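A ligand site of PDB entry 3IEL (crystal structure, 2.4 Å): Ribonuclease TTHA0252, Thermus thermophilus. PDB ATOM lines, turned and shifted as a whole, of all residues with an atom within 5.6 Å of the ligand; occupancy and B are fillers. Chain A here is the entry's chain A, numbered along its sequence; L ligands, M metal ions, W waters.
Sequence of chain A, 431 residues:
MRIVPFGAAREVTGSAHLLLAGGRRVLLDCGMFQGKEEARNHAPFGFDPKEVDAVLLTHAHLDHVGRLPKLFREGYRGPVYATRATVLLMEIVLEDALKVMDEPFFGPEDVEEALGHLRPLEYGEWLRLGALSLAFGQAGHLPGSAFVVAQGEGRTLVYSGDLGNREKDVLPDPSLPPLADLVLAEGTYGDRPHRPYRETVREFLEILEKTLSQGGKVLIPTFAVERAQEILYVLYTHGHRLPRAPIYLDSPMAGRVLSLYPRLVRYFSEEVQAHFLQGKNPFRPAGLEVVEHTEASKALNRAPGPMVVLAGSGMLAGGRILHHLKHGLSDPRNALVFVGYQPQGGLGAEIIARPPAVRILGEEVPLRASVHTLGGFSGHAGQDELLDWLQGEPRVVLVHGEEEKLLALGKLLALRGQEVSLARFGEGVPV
OE1 of Glu 402 sits at hydrogen-bond distance from N2 of the ligand (3.3 Å).
The side-chain hydroxyl (OG) of Ser 378 sits at hydrogen-bond distance from an oxygen (O8) of the ligand (2.6 Å).
An oxygen (O7) of the ligand is in hydrogen-bond range of the backbone NH (N) of Gly 379.
The backbone NH (N) of Tyr 341 lies within hydrogen-bond range of an oxygen (O9) of the ligand (2.8 Å).
An oxygen (O8) of the ligand is in hydrogen-bond range of the side-chain hydroxyl (OH) of Tyr 189.
The guanidinium group (NH1) of Arg 227 lies within salt-bridge range of an oxygen (O7) of the ligand (2.7 Å).
The side-chain amino group (NZ) of Lys 405 lies within hydrogen-bond range of an oxygen (O2) of the ligand (2.8 Å).
The side-chain hydroxyl (OG) of Ser 378 is in hydrogen-bond range of the backbone NH (N) of His 380, at 3.2 Å.
OG1 of Thr 188 is in hydrogen-bond range of ND1 of His 380, 3.5 Å away.
The side-chain amino group (NZ) of Lys 405 is in salt-bridge range of the side-chain carboxylate (OE1) of Glu 402, at 2.6 Å.
NE of Arg 227 sits close to O of Phe 377, 3.4 Å away.
OD2 of Asp 191 lies within salt-bridge range of NH1 of Arg 192 (2.7 Å).
NE2 of His 194 lies close to OG of Ser 378.
NE2 of His 400 lies close to O of Val 12 (3.0 Å).
NE2 of His 194 lies within hydrogen-bond range of O of His 380, 2.7 Å away.
Residues that only touch the ligand: Val 12, Thr 188, Gly 340, His 380, Arg 192 and Phe 223.
Hydrophobic or aromatic side chains within 4 Å of the ligand: Val 12, Tyr 189, Phe 223, Tyr 341 and His 380.
Water W1 bridges an oxygen (O4) of the ligand (2.4 Å) and a ring nitrogen (NE2) of His 380 (2.9 Å).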
ATOM      1  N   VAL A  12     -29.897   2.933 -33.493  1.00  0.00           N
ATOM      2  CA  VAL A  12     -30.028   4.303 -32.994  1.00  0.00           C
ATOM      3  C   VAL A  12     -30.304   5.444 -33.969  1.00  0.00           C
ATOM      4  O   VAL A  12     -30.543   6.558 -33.508  1.00  0.00           O
ATOM      5  CB  VAL A  12     -28.788   4.699 -32.148  1.00  0.00           C
ATOM      6  CG1 VAL A  12     -28.580   3.670 -31.038  1.00  0.00           C
ATOM      7  CG2 VAL A  12     -27.545   4.794 -33.021  1.00  0.00           C
ATOM      8  N   THR A  13     -30.283   5.212 -35.277  1.00  0.00           N
ATOM      9  CA  THR A  13     -30.562   6.302 -36.211  1.00  0.00           C
ATOM     10  C   THR A  13     -31.816   6.079 -37.080  1.00  0.00           C
ATOM     11  O   THR A  13     -32.434   5.011 -37.027  1.00  0.00           O
ATOM     12  CB  THR A  13     -29.352   6.583 -37.146  1.00  0.00           C
ATOM     13  OG1 THR A  13     -29.274   5.577 -38.167  1.00  0.00           O
ATOM     14  CG2 THR A  13     -28.053   6.565 -36.340  1.00  0.00           C
ATOM     15  N   ASP A  63     -30.141  12.849 -37.096  1.00  0.00           N
ATOM     16  CA  ASP A  63     -30.768  11.536 -37.075  1.00  0.00           C
ATOM     17  C   ASP A  63     -32.249  11.614 -36.683  1.00  0.00           C
ATOM     18  O   ASP A  63     -32.899  10.586 -36.486  1.00  0.00           O
ATOM     19  CB  ASP A  63     -29.986  10.556 -36.193  1.00  0.00           C
ATOM     20  CG  ASP A  63     -30.078  10.880 -34.715  1.00  0.00           C
ATOM     21  OD1 ASP A  63     -29.850  12.050 -34.329  1.00  0.00           O
ATOM     22  OD2 ASP A  63     -30.358   9.956 -33.924  1.00  0.00           O
ATOM     23  N   THR A 188     -31.032   4.104 -25.487  1.00  0.00           N
ATOM     24  CA  THR A 188     -29.645   4.150 -25.942  1.00  0.00           C
ATOM     25  C   THR A 188     -28.700   3.502 -24.913  1.00  0.00           C
ATOM     26  O   THR A 188     -27.874   2.647 -25.275  1.00  0.00           O
ATOM     27  CB  THR A 188     -29.185   5.598 -26.205  1.00  0.00           C
ATOM     28  OG1 THR A 188     -30.193   6.317 -26.945  1.00  0.00           O
ATOM     29  CG2 THR A 188     -27.898   5.583 -27.043  1.00  0.00           C
ATOM     30  N   TYR A 189     -28.832   3.906 -23.648  1.00  0.00           N
ATOM     31  CA  TYR A 189     -28.026   3.353 -22.564  1.00  0.00           C
ATOM     32  C   TYR A 189     -28.899   2.451 -21.679  1.00  0.00           C
ATOM     33  O   TYR A 189     -28.857   2.520 -20.442  1.00  0.00           O
ATOM     34  CB  TYR A 189     -27.406   4.471 -21.695  1.00  0.00           C
ATOM     35  CG  TYR A 189     -26.280   5.201 -22.373  1.00  0.00           C
ATOM     36  CD1 TYR A 189     -26.522   6.185 -23.346  1.00  0.00           C
ATOM     37  CD2 TYR A 189     -24.950   4.860 -22.093  1.00  0.00           C
ATOM     38  CE1 TYR A 189     -25.481   6.794 -24.017  1.00  0.00           C
ATOM     39  CE2 TYR A 189     -23.901   5.472 -22.768  1.00  0.00           C
ATOM     40  CZ  TYR A 189     -24.166   6.439 -23.730  1.00  0.00           C
ATOM     41  OH  TYR A 189     -23.124   6.995 -24.436  1.00  0.00           O
ATOM     42  N   ASP A 191     -28.544  -0.505 -21.007  1.00  0.00           N
ATOM     43  CA  ASP A 191     -27.694  -1.406 -20.236  1.00  0.00           C
ATOM     44  C   ASP A 191     -26.888  -0.802 -19.071  1.00  0.00           C
ATOM     45  O   ASP A 191     -26.415  -1.542 -18.206  1.00  0.00           O
ATOM     46  CB  ASP A 191     -26.695  -2.092 -21.167  1.00  0.00           C
ATOM     47  CG  ASP A 191     -25.793  -1.087 -21.876  1.00  0.00           C
ATOM     48  OD1 ASP A 191     -24.728  -1.490 -22.404  1.00  0.00           O
ATOM     49  OD2 ASP A 191     -26.144   0.113 -21.893  1.00  0.00           O
ATOM     50  N   ARG A 192     -26.710   0.512 -19.043  1.00  0.00           N
ATOM     51  CA  ARG A 192     -25.930   1.104 -17.952  1.00  0.00           C
ATOM     52  C   ARG A 192     -26.085   2.591 -17.656  1.00  0.00           C
ATOM     53  O   ARG A 192     -26.527   3.374 -18.495  1.00  0.00           O
ATOM     54  CB  ARG A 192     -24.432   0.800 -18.154  1.00  0.00           C
ATOM     55  CG  ARG A 192     -23.875   0.842 -19.595  1.00  0.00           C
ATOM     56  CD  ARG A 192     -23.610   2.247 -20.104  1.00  0.00           C
ATOM     57  NE  ARG A 192     -22.703   2.308 -21.262  1.00  0.00           N
ATOM     58  CZ  ARG A 192     -23.049   2.091 -22.531  1.00  0.00           C
ATOM     59  NH1 ARG A 192     -24.296   1.783 -22.875  1.00  0.00           N
ATOM     60  NH2 ARG A 192     -22.139   2.225 -23.488  1.00  0.00           N
ATOM     61  N   HIS A 194     -24.428   6.334 -16.388  1.00  0.00           N
ATOM     62  CA  HIS A 194     -23.174   7.006 -16.726  1.00  0.00           C
ATOM     63  C   HIS A 194     -22.411   7.331 -15.448  1.00  0.00           C
ATOM     64  O   HIS A 194     -22.973   7.332 -14.355  1.00  0.00           O
ATOM     65  CB  HIS A 194     -23.418   8.350 -17.414  1.00  0.00           C
ATOM     66  CG  HIS A 194     -24.346   8.284 -18.581  1.00  0.00           C
ATOM     67  ND1 HIS A 194     -24.000   7.718 -19.787  1.00  0.00           N
ATOM     68  CD2 HIS A 194     -25.594   8.792 -18.755  1.00  0.00           C
ATOM     69  CE1 HIS A 194     -24.994   7.879 -20.646  1.00  0.00           C
ATOM     70  NE2 HIS A 194     -25.971   8.533 -20.049  1.00  0.00           N
ATOM     71  N   PHE A 223     -19.080  16.787 -31.118  1.00  0.00           N
ATOM     72  CA  PHE A 223     -20.161  16.927 -32.072  1.00  0.00           C
ATOM     73  C   PHE A 223     -20.351  18.446 -32.153  1.00  0.00           C
ATOM     74  O   PHE A 223     -20.166  19.164 -31.155  1.00  0.00           O
ATOM     75  CB  PHE A 223     -21.446  16.276 -31.544  1.00  0.00           C
ATOM     76  CG  PHE A 223     -21.275  14.844 -31.107  1.00  0.00           C
ATOM     77  CD1 PHE A 223     -21.469  14.478 -29.771  1.00  0.00           C
ATOM     78  CD2 PHE A 223     -20.914  13.858 -32.015  1.00  0.00           C
ATOM     79  CE1 PHE A 223     -21.303  13.159 -29.350  1.00  0.00           C
ATOM     80  CE2 PHE A 223     -20.740  12.519 -31.615  1.00  0.00           C
ATOM     81  CZ  PHE A 223     -20.940  12.173 -30.280  1.00  0.00           C
ATOM     82  N   ARG A 227     -22.639  19.405 -27.899  1.00  0.00           N
ATOM     83  CA  ARG A 227     -21.551  18.926 -27.063  1.00  0.00           C
ATOM     84  C   ARG A 227     -20.424  19.961 -26.945  1.00  0.00           C
ATOM     85  O   ARG A 227     -19.990  20.289 -25.853  1.00  0.00           O
ATOM     86  CB  ARG A 227     -21.009  17.606 -27.639  1.00  0.00           C
ATOM     87  CG  ARG A 227     -20.043  16.810 -26.721  1.00  0.00           C
ATOM     88  CD  ARG A 227     -20.677  16.500 -25.361  1.00  0.00           C
ATOM     89  NE  ARG A 227     -22.025  15.951 -25.513  1.00  0.00           N
ATOM     90  CZ  ARG A 227     -22.300  14.660 -25.714  1.00  0.00           C
ATOM     91  NH1 ARG A 227     -23.573  14.292 -25.857  1.00  0.00           N
ATOM     92  NH2 ARG A 227     -21.338  13.751 -25.741  1.00  0.00           N
ATOM     93  N   MET A 315     -17.030  11.396 -33.809  1.00  0.00           N
ATOM     94  CA  MET A 315     -16.756   9.975 -33.751  1.00  0.00           C
ATOM     95  C   MET A 315     -15.600   9.580 -34.665  1.00  0.00           C
ATOM     96  O   MET A 315     -15.515   8.449 -35.134  1.00  0.00           O
ATOM     97  CB  MET A 315     -18.033   9.187 -34.071  1.00  0.00           C
ATOM     98  CG  MET A 315     -19.193   9.580 -33.166  1.00  0.00           C
ATOM     99  SD  MET A 315     -20.523   8.365 -32.940  1.00  0.00           S
ATOM    100  CE  MET A 315     -21.622   8.803 -34.289  1.00  0.00           C
ATOM    101  N   VAL A 339     -15.344  12.901 -25.023  1.00  0.00           N
ATOM    102  CA  VAL A 339     -16.428  13.449 -24.212  1.00  0.00           C
ATOM    103  C   VAL A 339     -17.721  13.036 -24.865  1.00  0.00           C
ATOM    104  O   VAL A 339     -18.783  13.544 -24.536  1.00  0.00           O
ATOM    105  CB  VAL A 339     -16.370  15.000 -24.148  1.00  0.00           C
ATOM    106  CG1 VAL A 339     -15.105  15.458 -23.450  1.00  0.00           C
ATOM    107  CG2 VAL A 339     -16.429  15.566 -25.557  1.00  0.00           C
ATOM    108  N   GLY A 340     -17.606  12.109 -25.816  1.00  0.00           N
ATOM    109  CA  GLY A 340     -18.754  11.602 -26.536  1.00  0.00           C
ATOM    110  C   GLY A 340     -18.525  10.143 -26.906  1.00  0.00           C
ATOM    111  O   GLY A 340     -17.402   9.748 -27.252  1.00  0.00           O
ATOM    112  N   TYR A 341     -19.583   9.349 -26.841  1.00  0.00           N
ATOM    113  CA  TYR A 341     -19.495   7.934 -27.169  1.00  0.00           C
ATOM    114  C   TYR A 341     -18.729   7.650 -28.458  1.00  0.00           C
ATOM    115  O   TYR A 341     -18.821   8.387 -29.432  1.00  0.00           O
ATOM    116  CB  TYR A 341     -20.922   7.353 -27.267  1.00  0.00           C
ATOM    117  CG  TYR A 341     -20.988   5.913 -27.752  1.00  0.00           C
ATOM    118  CD1 TYR A 341     -21.162   5.609 -29.098  1.00  0.00           C
ATOM    119  CD2 TYR A 341     -20.867   4.857 -26.854  1.00  0.00           C
ATOM    120  CE1 TYR A 341     -21.211   4.281 -29.543  1.00  0.00           C
ATOM    121  CE2 TYR A 341     -20.921   3.539 -27.277  1.00  0.00           C
ATOM    122  CZ  TYR A 341     -21.088   3.258 -28.619  1.00  0.00           C
ATOM    123  OH  TYR A 341     -21.148   1.939 -29.029  1.00  0.00           O
ATOM    124  N   GLY A 375     -17.353   9.398 -20.203  1.00  0.00           N
ATOM    125  CA  GLY A 375     -18.726   9.081 -20.566  1.00  0.00           C
ATOM    126  C   GLY A 375     -19.752   9.864 -19.802  1.00  0.00           C
ATOM    127  O   GLY A 375     -20.933   9.879 -20.166  1.00  0.00           O
ATOM    128  N   PHE A 377     -20.171  12.890 -19.789  1.00  0.00           N
ATOM    129  CA  PHE A 377     -20.594  14.058 -20.579  1.00  0.00           C
ATOM    130  C   PHE A 377     -21.692  13.667 -21.570  1.00  0.00           C
ATOM    131  O   PHE A 377     -22.104  14.490 -22.416  1.00  0.00           O
ATOM    132  CB  PHE A 377     -19.414  14.630 -21.378  1.00  0.00           C
ATOM    133  CG  PHE A 377     -18.580  15.610 -20.603  1.00  0.00           C
ATOM    134  CD1 PHE A 377     -17.250  15.323 -20.311  1.00  0.00           C
ATOM    135  CD2 PHE A 377     -19.115  16.829 -20.196  1.00  0.00           C
ATOM    136  CE1 PHE A 377     -16.454  16.244 -19.621  1.00  0.00           C
ATOM    137  CE2 PHE A 377     -18.335  17.766 -19.503  1.00  0.00           C
ATOM    138  CZ  PHE A 377     -17.004  17.469 -19.220  1.00  0.00           C
ATOM    139  N   SER A 378     -22.139  12.422 -21.495  1.00  0.00           N
ATOM    140  CA  SER A 378     -23.177  11.908 -22.391  1.00  0.00           C
ATOM    141  C   SER A 378     -24.438  12.756 -22.380  1.00  0.00           C
ATOM    142  O   SER A 378     -24.848  13.252 -21.333  1.00  0.00           O
ATOM    143  CB  SER A 378     -23.546  10.474 -22.001  1.00  0.00           C
ATOM    144  OG  SER A 378     -24.734  10.072 -22.661  1.00  0.00           O
ATOM    145  N   GLY A 379     -25.057  12.880 -23.555  1.00  0.00           N
ATOM    146  CA  GLY A 379     -26.280  13.658 -23.696  1.00  0.00           C
ATOM    147  C   GLY A 379     -27.585  12.843 -23.596  1.00  0.00           C
ATOM    148  O   GLY A 379     -28.679  13.387 -23.775  1.00  0.00           O
ATOM    149  N   HIS A 380     -27.463  11.566 -23.283  1.00  0.00           N
ATOM    150  CA  HIS A 380     -28.647  10.696 -23.141  1.00  0.00           C
ATOM    151  C   HIS A 380     -28.849  10.271 -21.698  1.00  0.00           C
ATOM    152  O   HIS A 380     -27.896  10.155 -20.938  1.00  0.00           O
ATOM    153  CB  HIS A 380     -28.475   9.446 -23.985  1.00  0.00           C
ATOM    154  CG  HIS A 380     -28.776   9.642 -25.432  1.00  0.00           C
ATOM    155  ND1 HIS A 380     -30.060   9.628 -25.938  1.00  0.00           N
ATOM    156  CD2 HIS A 380     -27.953   9.807 -26.503  1.00  0.00           C
ATOM    157  CE1 HIS A 380     -30.017   9.780 -27.251  1.00  0.00           C
ATOM    158  NE2 HIS A 380     -28.745   9.891 -27.612  1.00  0.00           N
ATOM    159  N   HIS A 400     -34.579   3.250 -30.598  1.00  0.00           N
ATOM    160  CA  HIS A 400     -33.347   3.995 -30.427  1.00  0.00           C
ATOM    161  C   HIS A 400     -32.303   3.317 -29.534  1.00  0.00           C
ATOM    162  O   HIS A 400     -31.934   3.833 -28.471  1.00  0.00           O
ATOM    163  CB  HIS A 400     -33.706   5.381 -29.872  1.00  0.00           C
ATOM    164  CG  HIS A 400     -32.684   6.423 -30.189  1.00  0.00           C
ATOM    165  ND1 HIS A 400     -31.463   6.476 -29.560  1.00  0.00           N
ATOM    166  CD2 HIS A 400     -32.683   7.400 -31.117  1.00  0.00           C
ATOM    167  CE1 HIS A 400     -30.739   7.435 -30.103  1.00  0.00           C
ATOM    168  NE2 HIS A 400     -31.454   8.012 -31.051  1.00  0.00           N
ATOM    169  N   GLU A 402     -29.237  -0.346 -29.472  1.00  0.00           N
ATOM    170  CA  GLU A 402     -28.777  -1.634 -29.949  1.00  0.00           C
ATOM    171  C   GLU A 402     -29.643  -2.659 -29.250  1.00  0.00           C
ATOM    172  O   GLU A 402     -30.038  -2.457 -28.097  1.00  0.00           O
ATOM    173  CB  GLU A 402     -27.311  -1.833 -29.589  1.00  0.00           C
ATOM    174  CG  GLU A 402     -26.367  -1.044 -30.460  1.00  0.00           C
ATOM    175  CD  GLU A 402     -25.108  -0.627 -29.720  1.00  0.00           C
ATOM    176  OE1 GLU A 402     -25.240   0.190 -28.778  1.00  0.00           O
ATOM    177  OE2 GLU A 402     -24.015  -1.106 -30.064  1.00  0.00           O
ATOM    178  N   LYS A 405     -28.702  -3.611 -25.645  1.00  0.00           N
ATOM    179  CA  LYS A 405     -28.865  -2.520 -24.693  1.00  0.00           C
ATOM    180  C   LYS A 405     -30.347  -2.405 -24.392  1.00  0.00           C
ATOM    181  O   LYS A 405     -30.758  -2.229 -23.240  1.00  0.00           O
ATOM    182  CB  LYS A 405     -28.377  -1.186 -25.279  1.00  0.00           C
ATOM    183  CG  LYS A 405     -27.019  -1.212 -25.948  1.00  0.00           C
ATOM    184  CD  LYS A 405     -25.927  -1.484 -24.976  1.00  0.00           C
ATOM    185  CE  LYS A 405     -24.575  -1.417 -25.647  1.00  0.00           C
ATOM    186  NZ  LYS A 405     -24.384  -0.105 -26.298  1.00  0.00           N
HETATM  187  N1  LIG L   1     -24.699   5.802 -29.019  1.00  0.00           N
HETATM  188  C1  LIG L   1     -24.713   4.400 -29.485  1.00  0.00           C
HETATM  189  N2  LIG L   1     -24.539   3.393 -28.560  1.00  0.00           N
HETATM  190  C2  LIG L   1     -24.348   3.671 -27.215  1.00  0.00           C
HETATM  191  C3  LIG L   1     -24.325   5.003 -26.720  1.00  0.00           C
HETATM  192  C4  LIG L   1     -24.499   6.062 -27.664  1.00  0.00           C
HETATM  193  O1  LIG L   1     -24.878   4.085 -30.705  1.00  0.00           O
HETATM  194  O2  LIG L   1     -24.207   2.687 -26.443  1.00  0.00           O
HETATM  195  C5  LIG L   1     -24.903   6.812 -30.106  1.00  0.00           C
HETATM  196  C6  LIG L   1     -26.177   7.630 -30.203  1.00  0.00           C
HETATM  197  O3  LIG L   1     -26.700   7.690 -31.552  1.00  0.00           O
HETATM  198  C7  LIG L   1     -25.788   9.015 -29.671  1.00  0.00           C
HETATM  199  C8  LIG L   1     -24.272   9.093 -29.887  1.00  0.00           C
HETATM  200  O4  LIG L   1     -26.428  10.113 -30.332  1.00  0.00           O
HETATM  201  O5  LIG L   1     -23.794   7.740 -30.114  1.00  0.00           O
HETATM  202  C9  LIG L   1     -23.465   9.760 -28.732  1.00  0.00           C
HETATM  203  O6  LIG L   1     -24.132   9.708 -27.434  1.00  0.00           O
HETATM  204  P1  LIG L   1     -23.581  10.404 -26.227  1.00  0.00           P
HETATM  205  O7  LIG L   1     -24.210  11.707 -26.057  1.00  0.00           O
HETATM  206  O8  LIG L   1     -23.752   9.414 -24.949  1.00  0.00           O
HETATM  207  O9  LIG L   1     -22.095  10.602 -26.376  1.00  0.00           O
HETATM  208 ZN    ZN M   1     -29.802  13.108 -30.309  1.00  0.00          ZN
HETATM  209 ZN    ZN M   2     -31.244  10.346 -31.530  1.00  0.00          ZN
HETATM  210  O   HOH W   1     -28.512  11.356 -30.143  1.00  0.00           O
